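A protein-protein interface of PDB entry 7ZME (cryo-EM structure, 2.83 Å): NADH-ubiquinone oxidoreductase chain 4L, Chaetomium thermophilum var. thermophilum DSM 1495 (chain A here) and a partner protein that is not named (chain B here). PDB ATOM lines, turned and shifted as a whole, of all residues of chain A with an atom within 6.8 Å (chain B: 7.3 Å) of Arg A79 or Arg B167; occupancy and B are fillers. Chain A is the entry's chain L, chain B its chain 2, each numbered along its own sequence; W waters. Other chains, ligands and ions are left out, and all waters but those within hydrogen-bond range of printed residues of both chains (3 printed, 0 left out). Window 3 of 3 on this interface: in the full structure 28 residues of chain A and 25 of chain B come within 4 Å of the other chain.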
ATOM      1  N   LEU A  74     -19.876   6.329  -9.124  1.00  0.00           N
ATOM      2  CA  LEU A  74     -19.810   5.673 -10.428  1.00  0.00           C
ATOM      3  C   LEU A  74     -19.429   6.649 -11.529  1.00  0.00           C
ATOM      4  O   LEU A  74     -18.623   6.318 -12.405  1.00  0.00           O
ATOM      5  CB  LEU A  74     -21.138   5.007 -10.771  1.00  0.00           C
ATOM      6  CG  LEU A  74     -21.424   3.673 -10.113  1.00  0.00           C
ATOM      7  CD1 LEU A  74     -22.820   3.222 -10.462  1.00  0.00           C
ATOM      8  CD2 LEU A  74     -20.404   2.698 -10.648  1.00  0.00           C
ATOM      9  N   VAL A  75     -20.012   7.847 -11.518  1.00  0.00           N
ATOM     10  CA  VAL A  75     -19.689   8.829 -12.546  1.00  0.00           C
ATOM     11  C   VAL A  75     -18.205   9.167 -12.499  1.00  0.00           C
ATOM     12  O   VAL A  75     -17.521   9.179 -13.527  1.00  0.00           O
ATOM     13  CB  VAL A  75     -20.568  10.081 -12.385  1.00  0.00           C
ATOM     14  CG1 VAL A  75     -20.001  11.238 -13.179  1.00  0.00           C
ATOM     15  CG2 VAL A  75     -21.973   9.782 -12.828  1.00  0.00           C
ATOM     16  N   ALA A  76     -17.669   9.348 -11.292  1.00  0.00           N
ATOM     17  CA  ALA A  76     -16.224   9.599 -11.116  1.00  0.00           C
ATOM     18  C   ALA A  76     -15.404   8.451 -11.707  1.00  0.00           C
ATOM     19  O   ALA A  76     -14.467   8.728 -12.465  1.00  0.00           O
ATOM     20  CB  ALA A  76     -15.961   9.779  -9.648  1.00  0.00           C
ATOM     21  N   PHE A  77     -15.728   7.217 -11.342  1.00  0.00           N
ATOM     22  CA  PHE A  77     -15.021   6.008 -11.830  1.00  0.00           C
ATOM     23  C   PHE A  77     -15.144   5.859 -13.348  1.00  0.00           C
ATOM     24  O   PHE A  77     -14.109   5.611 -13.966  1.00  0.00           O
ATOM     25  CB  PHE A  77     -15.620   4.802 -11.098  1.00  0.00           C
ATOM     26  CG  PHE A  77     -15.100   3.438 -11.466  1.00  0.00           C
ATOM     27  CD1 PHE A  77     -13.935   2.949 -10.900  1.00  0.00           C
ATOM     28  CD2 PHE A  77     -15.807   2.622 -12.333  1.00  0.00           C
ATOM     29  CE1 PHE A  77     -13.471   1.685 -11.223  1.00  0.00           C
ATOM     30  CE2 PHE A  77     -15.340   1.358 -12.654  1.00  0.00           C
ATOM     31  CZ  PHE A  77     -14.177   0.892 -12.095  1.00  0.00           C
ATOM     32  N   TYR A  78     -16.343   6.021 -13.918  1.00  0.00           N
ATOM     33  CA  TYR A  78     -16.573   5.869 -15.380  1.00  0.00           C
ATOM     34  C   TYR A  78     -15.793   6.938 -16.144  1.00  0.00           C
ATOM     35  O   TYR A  78     -15.293   6.658 -17.222  1.00  0.00           O
ATOM     36  CB  TYR A  78     -18.070   5.891 -15.688  1.00  0.00           C
ATOM     37  CG  TYR A  78     -18.434   5.743 -17.142  1.00  0.00           C
ATOM     38  CD1 TYR A  78     -18.572   4.492 -17.713  1.00  0.00           C
ATOM     39  CD2 TYR A  78     -18.647   6.851 -17.944  1.00  0.00           C
ATOM     40  CE1 TYR A  78     -18.910   4.343 -19.046  1.00  0.00           C
ATOM     41  CE2 TYR A  78     -18.984   6.720 -19.278  1.00  0.00           C
ATOM     42  CZ  TYR A  78     -19.117   5.461 -19.830  1.00  0.00           C
ATOM     43  OH  TYR A  78     -19.449   5.320 -21.143  1.00  0.00           O
ATOM     44  N   ARG A  79     -15.698   8.138 -15.591  1.00  0.00           N
ATOM     45  CA  ARG A  79     -15.035   9.257 -16.289  1.00  0.00           C
ATOM     46  C   ARG A  79     -13.601   8.855 -16.578  1.00  0.00           C
ATOM     47  O   ARG A  79     -13.066   9.270 -17.614  1.00  0.00           O
ATOM     48  CB  ARG A  79     -15.139  10.539 -15.463  1.00  0.00           C
ATOM     49  CG  ARG A  79     -16.423  11.311 -15.708  1.00  0.00           C
ATOM     50  CD  ARG A  79     -16.576  12.511 -14.803  1.00  0.00           C
ATOM     51  NE  ARG A  79     -17.801  13.225 -15.127  1.00  0.00           N
ATOM     52  CZ  ARG A  79     -18.192  14.340 -14.530  1.00  0.00           C
ATOM     53  NH1 ARG A  79     -19.318  14.924 -14.896  1.00  0.00           N
ATOM     54  NH2 ARG A  79     -17.450  14.875 -13.576  1.00  0.00           N
ATOM     55  N   LEU A  80     -13.001   8.102 -15.667  1.00  0.00           N
ATOM     56  CA  LEU A  80     -11.600   7.691 -15.855  1.00  0.00           C
ATOM     57  C   LEU A  80     -11.503   6.303 -16.513  1.00  0.00           C
ATOM     58  O   LEU A  80     -10.797   6.191 -17.520  1.00  0.00           O
ATOM     59  CB  LEU A  80     -10.955   7.777 -14.476  1.00  0.00           C
ATOM     60  CG  LEU A  80     -11.044   9.156 -13.826  1.00  0.00           C
ATOM     61  CD1 LEU A  80     -10.691   9.099 -12.354  1.00  0.00           C
ATOM     62  CD2 LEU A  80     -10.161  10.160 -14.545  1.00  0.00           C
ATOM     63  N   ARG A  81     -12.193   5.296 -15.989  1.00  0.00           N
ATOM     64  CA  ARG A  81     -12.138   3.915 -16.528  1.00  0.00           C
ATOM     65  C   ARG A  81     -12.827   3.791 -17.889  1.00  0.00           C
ATOM     66  O   ARG A  81     -12.311   3.035 -18.730  1.00  0.00           O
ATOM     67  CB  ARG A  81     -12.666   2.909 -15.500  1.00  0.00           C
ATOM     68  CG  ARG A  81     -12.427   1.463 -15.905  1.00  0.00           C
ATOM     69  CD  ARG A  81     -12.003   0.601 -14.736  1.00  0.00           C
ATOM     70  NE  ARG A  81     -11.028   1.274 -13.892  1.00  0.00           N
ATOM     71  CZ  ARG A  81      -9.713   1.137 -14.006  1.00  0.00           C
ATOM     72  NH1 ARG A  81      -9.208   0.345 -14.935  1.00  0.00           N
ATOM     73  NH2 ARG A  81      -8.907   1.794 -13.191  1.00  0.00           N
ATOM     74  N   GLY A  82     -13.978   4.438 -18.072  1.00  0.00           N
ATOM     75  CA  GLY A  82     -14.721   4.389 -19.348  1.00  0.00           C
ATOM     76  C   GLY A  82     -15.620   3.174 -19.481  1.00  0.00           C
ATOM     77  O   GLY A  82     -16.269   3.040 -20.526  1.00  0.00           O
ATOM     78  N   SER A  83     -15.644   2.301 -18.485  1.00  0.00           N
ATOM     79  CA  SER A  83     -16.573   1.149 -18.486  1.00  0.00           C
ATOM     80  C   SER A  83     -16.971   0.888 -17.041  1.00  0.00           C
ATOM     81  O   SER A  83     -16.119   1.113 -16.164  1.00  0.00           O
ATOM     82  CB  SER A  83     -15.903  -0.064 -19.063  1.00  0.00           C
ATOM     83  OG  SER A  83     -16.627  -1.242 -18.764  1.00  0.00           O
ATOM     84  N   ILE A  84     -18.243   0.603 -16.766  1.00  0.00           N
ATOM     85  CA  ILE A  84     -18.628   0.238 -15.372  1.00  0.00           C
ATOM     86  C   ILE A  84     -19.114  -1.200 -15.434  1.00  0.00           C
ATOM     87  O   ILE A  84     -19.991  -1.574 -14.650  1.00  0.00           O
ATOM     88  CB  ILE A  84     -19.663   1.194 -14.755  1.00  0.00           C
ATOM     89  CG1 ILE A  84     -20.976   1.229 -15.540  1.00  0.00           C
ATOM     90  CG2 ILE A  84     -19.082   2.585 -14.561  1.00  0.00           C
ATOM     91  CD1 ILE A  84     -22.196   1.261 -14.660  1.00  0.00           C
ATOM     92  N   ILE B 122      -8.299  21.005  -2.694  1.00  0.00           N
ATOM     93  CA  ILE B 122      -9.705  20.557  -2.458  1.00  0.00           C
ATOM     94  C   ILE B 122     -10.276  21.438  -1.353  1.00  0.00           C
ATOM     95  O   ILE B 122      -9.688  21.462  -0.271  1.00  0.00           O
ATOM     96  CB  ILE B 122      -9.799  19.045  -2.170  1.00  0.00           C
ATOM     97  CG1 ILE B 122      -9.069  18.231  -3.239  1.00  0.00           C
ATOM     98  CG2 ILE B 122     -11.246  18.607  -2.013  1.00  0.00           C
ATOM     99  CD1 ILE B 122      -8.955  16.768  -2.919  1.00  0.00           C
ATOM    100  N   SER B 163     -12.612   8.956   0.052  1.00  0.00           N
ATOM    101  CA  SER B 163     -11.782   8.030  -0.751  1.00  0.00           C
ATOM    102  C   SER B 163     -11.896   8.427  -2.228  1.00  0.00           C
ATOM    103  O   SER B 163     -10.932   8.184  -2.957  1.00  0.00           O
ATOM    104  CB  SER B 163     -12.221   6.615  -0.528  1.00  0.00           C
ATOM    105  OG  SER B 163     -12.072   6.246   0.833  1.00  0.00           O
ATOM    106  N   THR B 164     -12.983   9.086  -2.635  1.00  0.00           N
ATOM    107  CA  THR B 164     -13.211   9.478  -4.050  1.00  0.00           C
ATOM    108  C   THR B 164     -12.966  10.975  -4.235  1.00  0.00           C
ATOM    109  O   THR B 164     -13.184  11.461  -5.340  1.00  0.00           O
ATOM    110  CB  THR B 164     -14.660   9.146  -4.437  1.00  0.00           C
ATOM    111  OG1 THR B 164     -15.083   8.058  -3.615  1.00  0.00           O
ATOM    112  CG2 THR B 164     -14.840   8.784  -5.894  1.00  0.00           C
ATOM    113  N   ILE B 165     -12.528  11.674  -3.197  1.00  0.00           N
ATOM    114  CA  ILE B 165     -12.385  13.160  -3.263  1.00  0.00           C
ATOM    115  C   ILE B 165     -11.353  13.566  -4.317  1.00  0.00           C
ATOM    116  O   ILE B 165     -11.471  14.677  -4.855  1.00  0.00           O
ATOM    117  CB  ILE B 165     -12.198  13.802  -1.871  1.00  0.00           C
ATOM    118  CG1 ILE B 165     -12.901  15.159  -1.783  1.00  0.00           C
ATOM    119  CG2 ILE B 165     -10.740  13.878  -1.450  1.00  0.00           C
ATOM    120  CD1 ILE B 165     -13.119  15.646  -0.376  1.00  0.00           C
ATOM    121  N   TYR B 166     -10.343  12.737  -4.559  1.00  0.00           N
ATOM    122  CA  TYR B 166      -9.371  13.003  -5.651  1.00  0.00           C
ATOM    123  C   TYR B 166     -10.016  12.462  -6.924  1.00  0.00           C
ATOM    124  O   TYR B 166      -9.697  11.335  -7.307  1.00  0.00           O
ATOM    125  CB  TYR B 166      -8.013  12.393  -5.310  1.00  0.00           C
ATOM    126  CG  TYR B 166      -7.196  13.167  -4.310  1.00  0.00           C
ATOM    127  CD1 TYR B 166      -7.567  13.231  -2.979  1.00  0.00           C
ATOM    128  CD2 TYR B 166      -6.037  13.818  -4.692  1.00  0.00           C
ATOM    129  CE1 TYR B 166      -6.815  13.929  -2.052  1.00  0.00           C
ATOM    130  CE2 TYR B 166      -5.270  14.521  -3.779  1.00  0.00           C
ATOM    131  CZ  TYR B 166      -5.662  14.575  -2.456  1.00  0.00           C
ATOM    132  OH  TYR B 166      -4.916  15.261  -1.549  1.00  0.00           O
ATOM    133  N   ARG B 167     -10.906  13.241  -7.535  1.00  0.00           N
ATOM    134  CA  ARG B 167     -11.721  12.824  -8.706  1.00  0.00           C
ATOM    135  C   ARG B 167     -10.868  12.538  -9.935  1.00  0.00           C
ATOM    136  O   ARG B 167     -11.258  11.674 -10.712  1.00  0.00           O
ATOM    137  CB  ARG B 167     -12.696  13.970  -8.972  1.00  0.00           C
ATOM    138  CG  ARG B 167     -12.063  15.340  -8.789  1.00  0.00           C
ATOM    139  CD  ARG B 167     -13.123  16.391  -8.995  1.00  0.00           C
ATOM    140  NE  ARG B 167     -13.778  16.167 -10.268  1.00  0.00           N
ATOM    141  CZ  ARG B 167     -14.995  16.600 -10.547  1.00  0.00           C
ATOM    142  NH1 ARG B 167     -15.527  16.367 -11.733  1.00  0.00           N
ATOM    143  NH2 ARG B 167     -15.676  17.254  -9.629  1.00  0.00           N
ATOM    144  N   ASN B 168      -9.769  13.263 -10.104  1.00  0.00           N
ATOM    145  CA  ASN B 168      -8.908  13.136 -11.305  1.00  0.00           C
ATOM    146  C   ASN B 168      -7.950  11.958 -11.126  1.00  0.00           C
ATOM    147  O   ASN B 168      -7.135  11.733 -12.032  1.00  0.00           O
ATOM    148  CB  ASN B 168      -8.211  14.466 -11.576  1.00  0.00           C
ATOM    149  CG  ASN B 168      -9.173  15.630 -11.606  1.00  0.00           C
ATOM    150  OD1 ASN B 168     -10.356  15.456 -11.884  1.00  0.00           O
ATOM    151  ND2 ASN B 168      -8.675  16.823 -11.328  1.00  0.00           N
ATOM    152  N   SER B 169      -8.038  11.250  -9.997  1.00  0.00           N
ATOM    153  CA  SER B 169      -7.200  10.044  -9.770  1.00  0.00           C
ATOM    154  C   SER B 169      -7.996   8.771 -10.056  1.00  0.00           C
ATOM    155  O   SER B 169      -9.000   8.558  -9.370  1.00  0.00           O
ATOM    156  CB  SER B 169      -6.666  10.029  -8.374  1.00  0.00           C
ATOM    157  OG  SER B 169      -6.059   8.783  -8.075  1.00  0.00           O
ATOM    158  N   GLU B 170      -7.552   7.952 -11.016  1.00  0.00           N
ATOM    159  CA  GLU B 170      -8.214   6.648 -11.308  1.00  0.00           C
ATOM    160  C   GLU B 170      -8.064   5.700 -10.114  1.00  0.00           C
ATOM    161  O   GLU B 170      -9.001   4.931  -9.856  1.00  0.00           O
ATOM    162  CB  GLU B 170      -7.722   6.039 -12.622  1.00  0.00           C
ATOM    163  CG  GLU B 170      -6.261   5.624 -12.628  1.00  0.00           C
ATOM    164  CD  GLU B 170      -5.261   6.675 -13.081  1.00  0.00           C
ATOM    165  OE1 GLU B 170      -5.588   7.878 -13.015  1.00  0.00           O
ATOM    166  OE2 GLU B 170      -4.158   6.286 -13.510  1.00  0.00           O
ATOM    167  N   SER B 172      -7.842   6.464  -6.855  1.00  0.00           N
ATOM    168  CA  SER B 172      -8.747   6.877  -5.751  1.00  0.00           C
ATOM    169  C   SER B 172     -10.196   6.522  -6.082  1.00  0.00           C
ATOM    170  O   SER B 172     -10.926   6.111  -5.175  1.00  0.00           O
ATOM    171  CB  SER B 172      -8.572   8.320  -5.394  1.00  0.00           C
ATOM    172  OG  SER B 172      -7.207   8.601  -5.146  1.00  0.00           O
ATOM    173  N   THR B 173     -10.591   6.694  -7.337  1.00  0.00           N
ATOM    174  CA  THR B 173     -11.987   6.401  -7.740  1.00  0.00           C
ATOM    175  C   THR B 173     -12.236   4.912  -7.535  1.00  0.00           C
ATOM    176  O   THR B 173     -13.355   4.553  -7.180  1.00  0.00           O
ATOM    177  CB  THR B 173     -12.316   6.972  -9.125  1.00  0.00           C
ATOM    178  OG1 THR B 173     -11.312   6.553 -10.046  1.00  0.00           O
ATOM    179  CG2 THR B 173     -12.407   8.481  -9.117  1.00  0.00           C
HETATM  180  O   HOH W   1     -15.619  13.133 -11.373  1.00  0.00           O
HETATM  181  O   HOH W   2     -11.602   4.932 -12.289  1.00  0.00           O
HETATM  182  O   HOH W   3     -13.769  11.698 -12.426  1.00  0.00           O
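NH1 of Arg B167 lies close to NH2 of Arg A79.
The side-chain hydroxyl (OG) of Ser B169 is in hydrogen-bond range of the side-chain hydroxyl (OG) of Ser B172 (3.2 Å). The backbone carbonyl oxygen (O) of Ser B169 lies within hydrogen-bond range of the side-chain hydroxyl (OG1) of Thr B173, at 3.1 Å. The side-chain hydroxyl of Thr B173 lies within hydrogen-bond range of the backbone carbonyl oxygen of Glu B170 (2.8 Å).
Among the printed residues, pairs that only touch across the chains: Leu A80 with Arg B167 (3.1 Å), Leu A80 with Ser B169 (3.5 Å), Leu A80 with Thr B173 (3.5 Å), Leu A80 with Glu B170 (3.6 Å), Ala A76 with Thr B173 (3.8 Å) and Phe A77 with Thr B173 (3.9 Å).
Printed residues of chain B within 4 Å of Ala A76: Thr B173. Of the printed residues of chain B, Phe A77 touches Thr B173. Arg A79 touches just one residue of chain B: Arg B167. Of the printed residues of chain B, Leu A80 touches Arg B167, Ser B169, Glu B170 and Thr B173. Ile B122 touches none of the printed residues of chain A. Arg B167 touches just these residues of chain A: Arg A79 (3.1 Å) and Leu A80 (3.1 Å). Of the printed residues of chain A, Ser B169 touches Leu A80.
Printed residues of chain B that touch a printed residue of chain A: Arg B167, Ser B169, Glu B170 and Thr B173. Among the printed residues, 7 pairs touch across the chains.
Water W2 bridges OG1 of Thr B173 (2.8 Å) and O of Phe A77 (3.1 Å). Water W3 lies within hydrogen-bond range of the backbone carbonyl oxygen (O) of Arg B167 (3.0 Å) and the backbone carbonyl oxygen (O) of Ala A76 (3.1 Å). Water W1 bridges NH1 of Arg B167 and NH2 of Arg A79.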
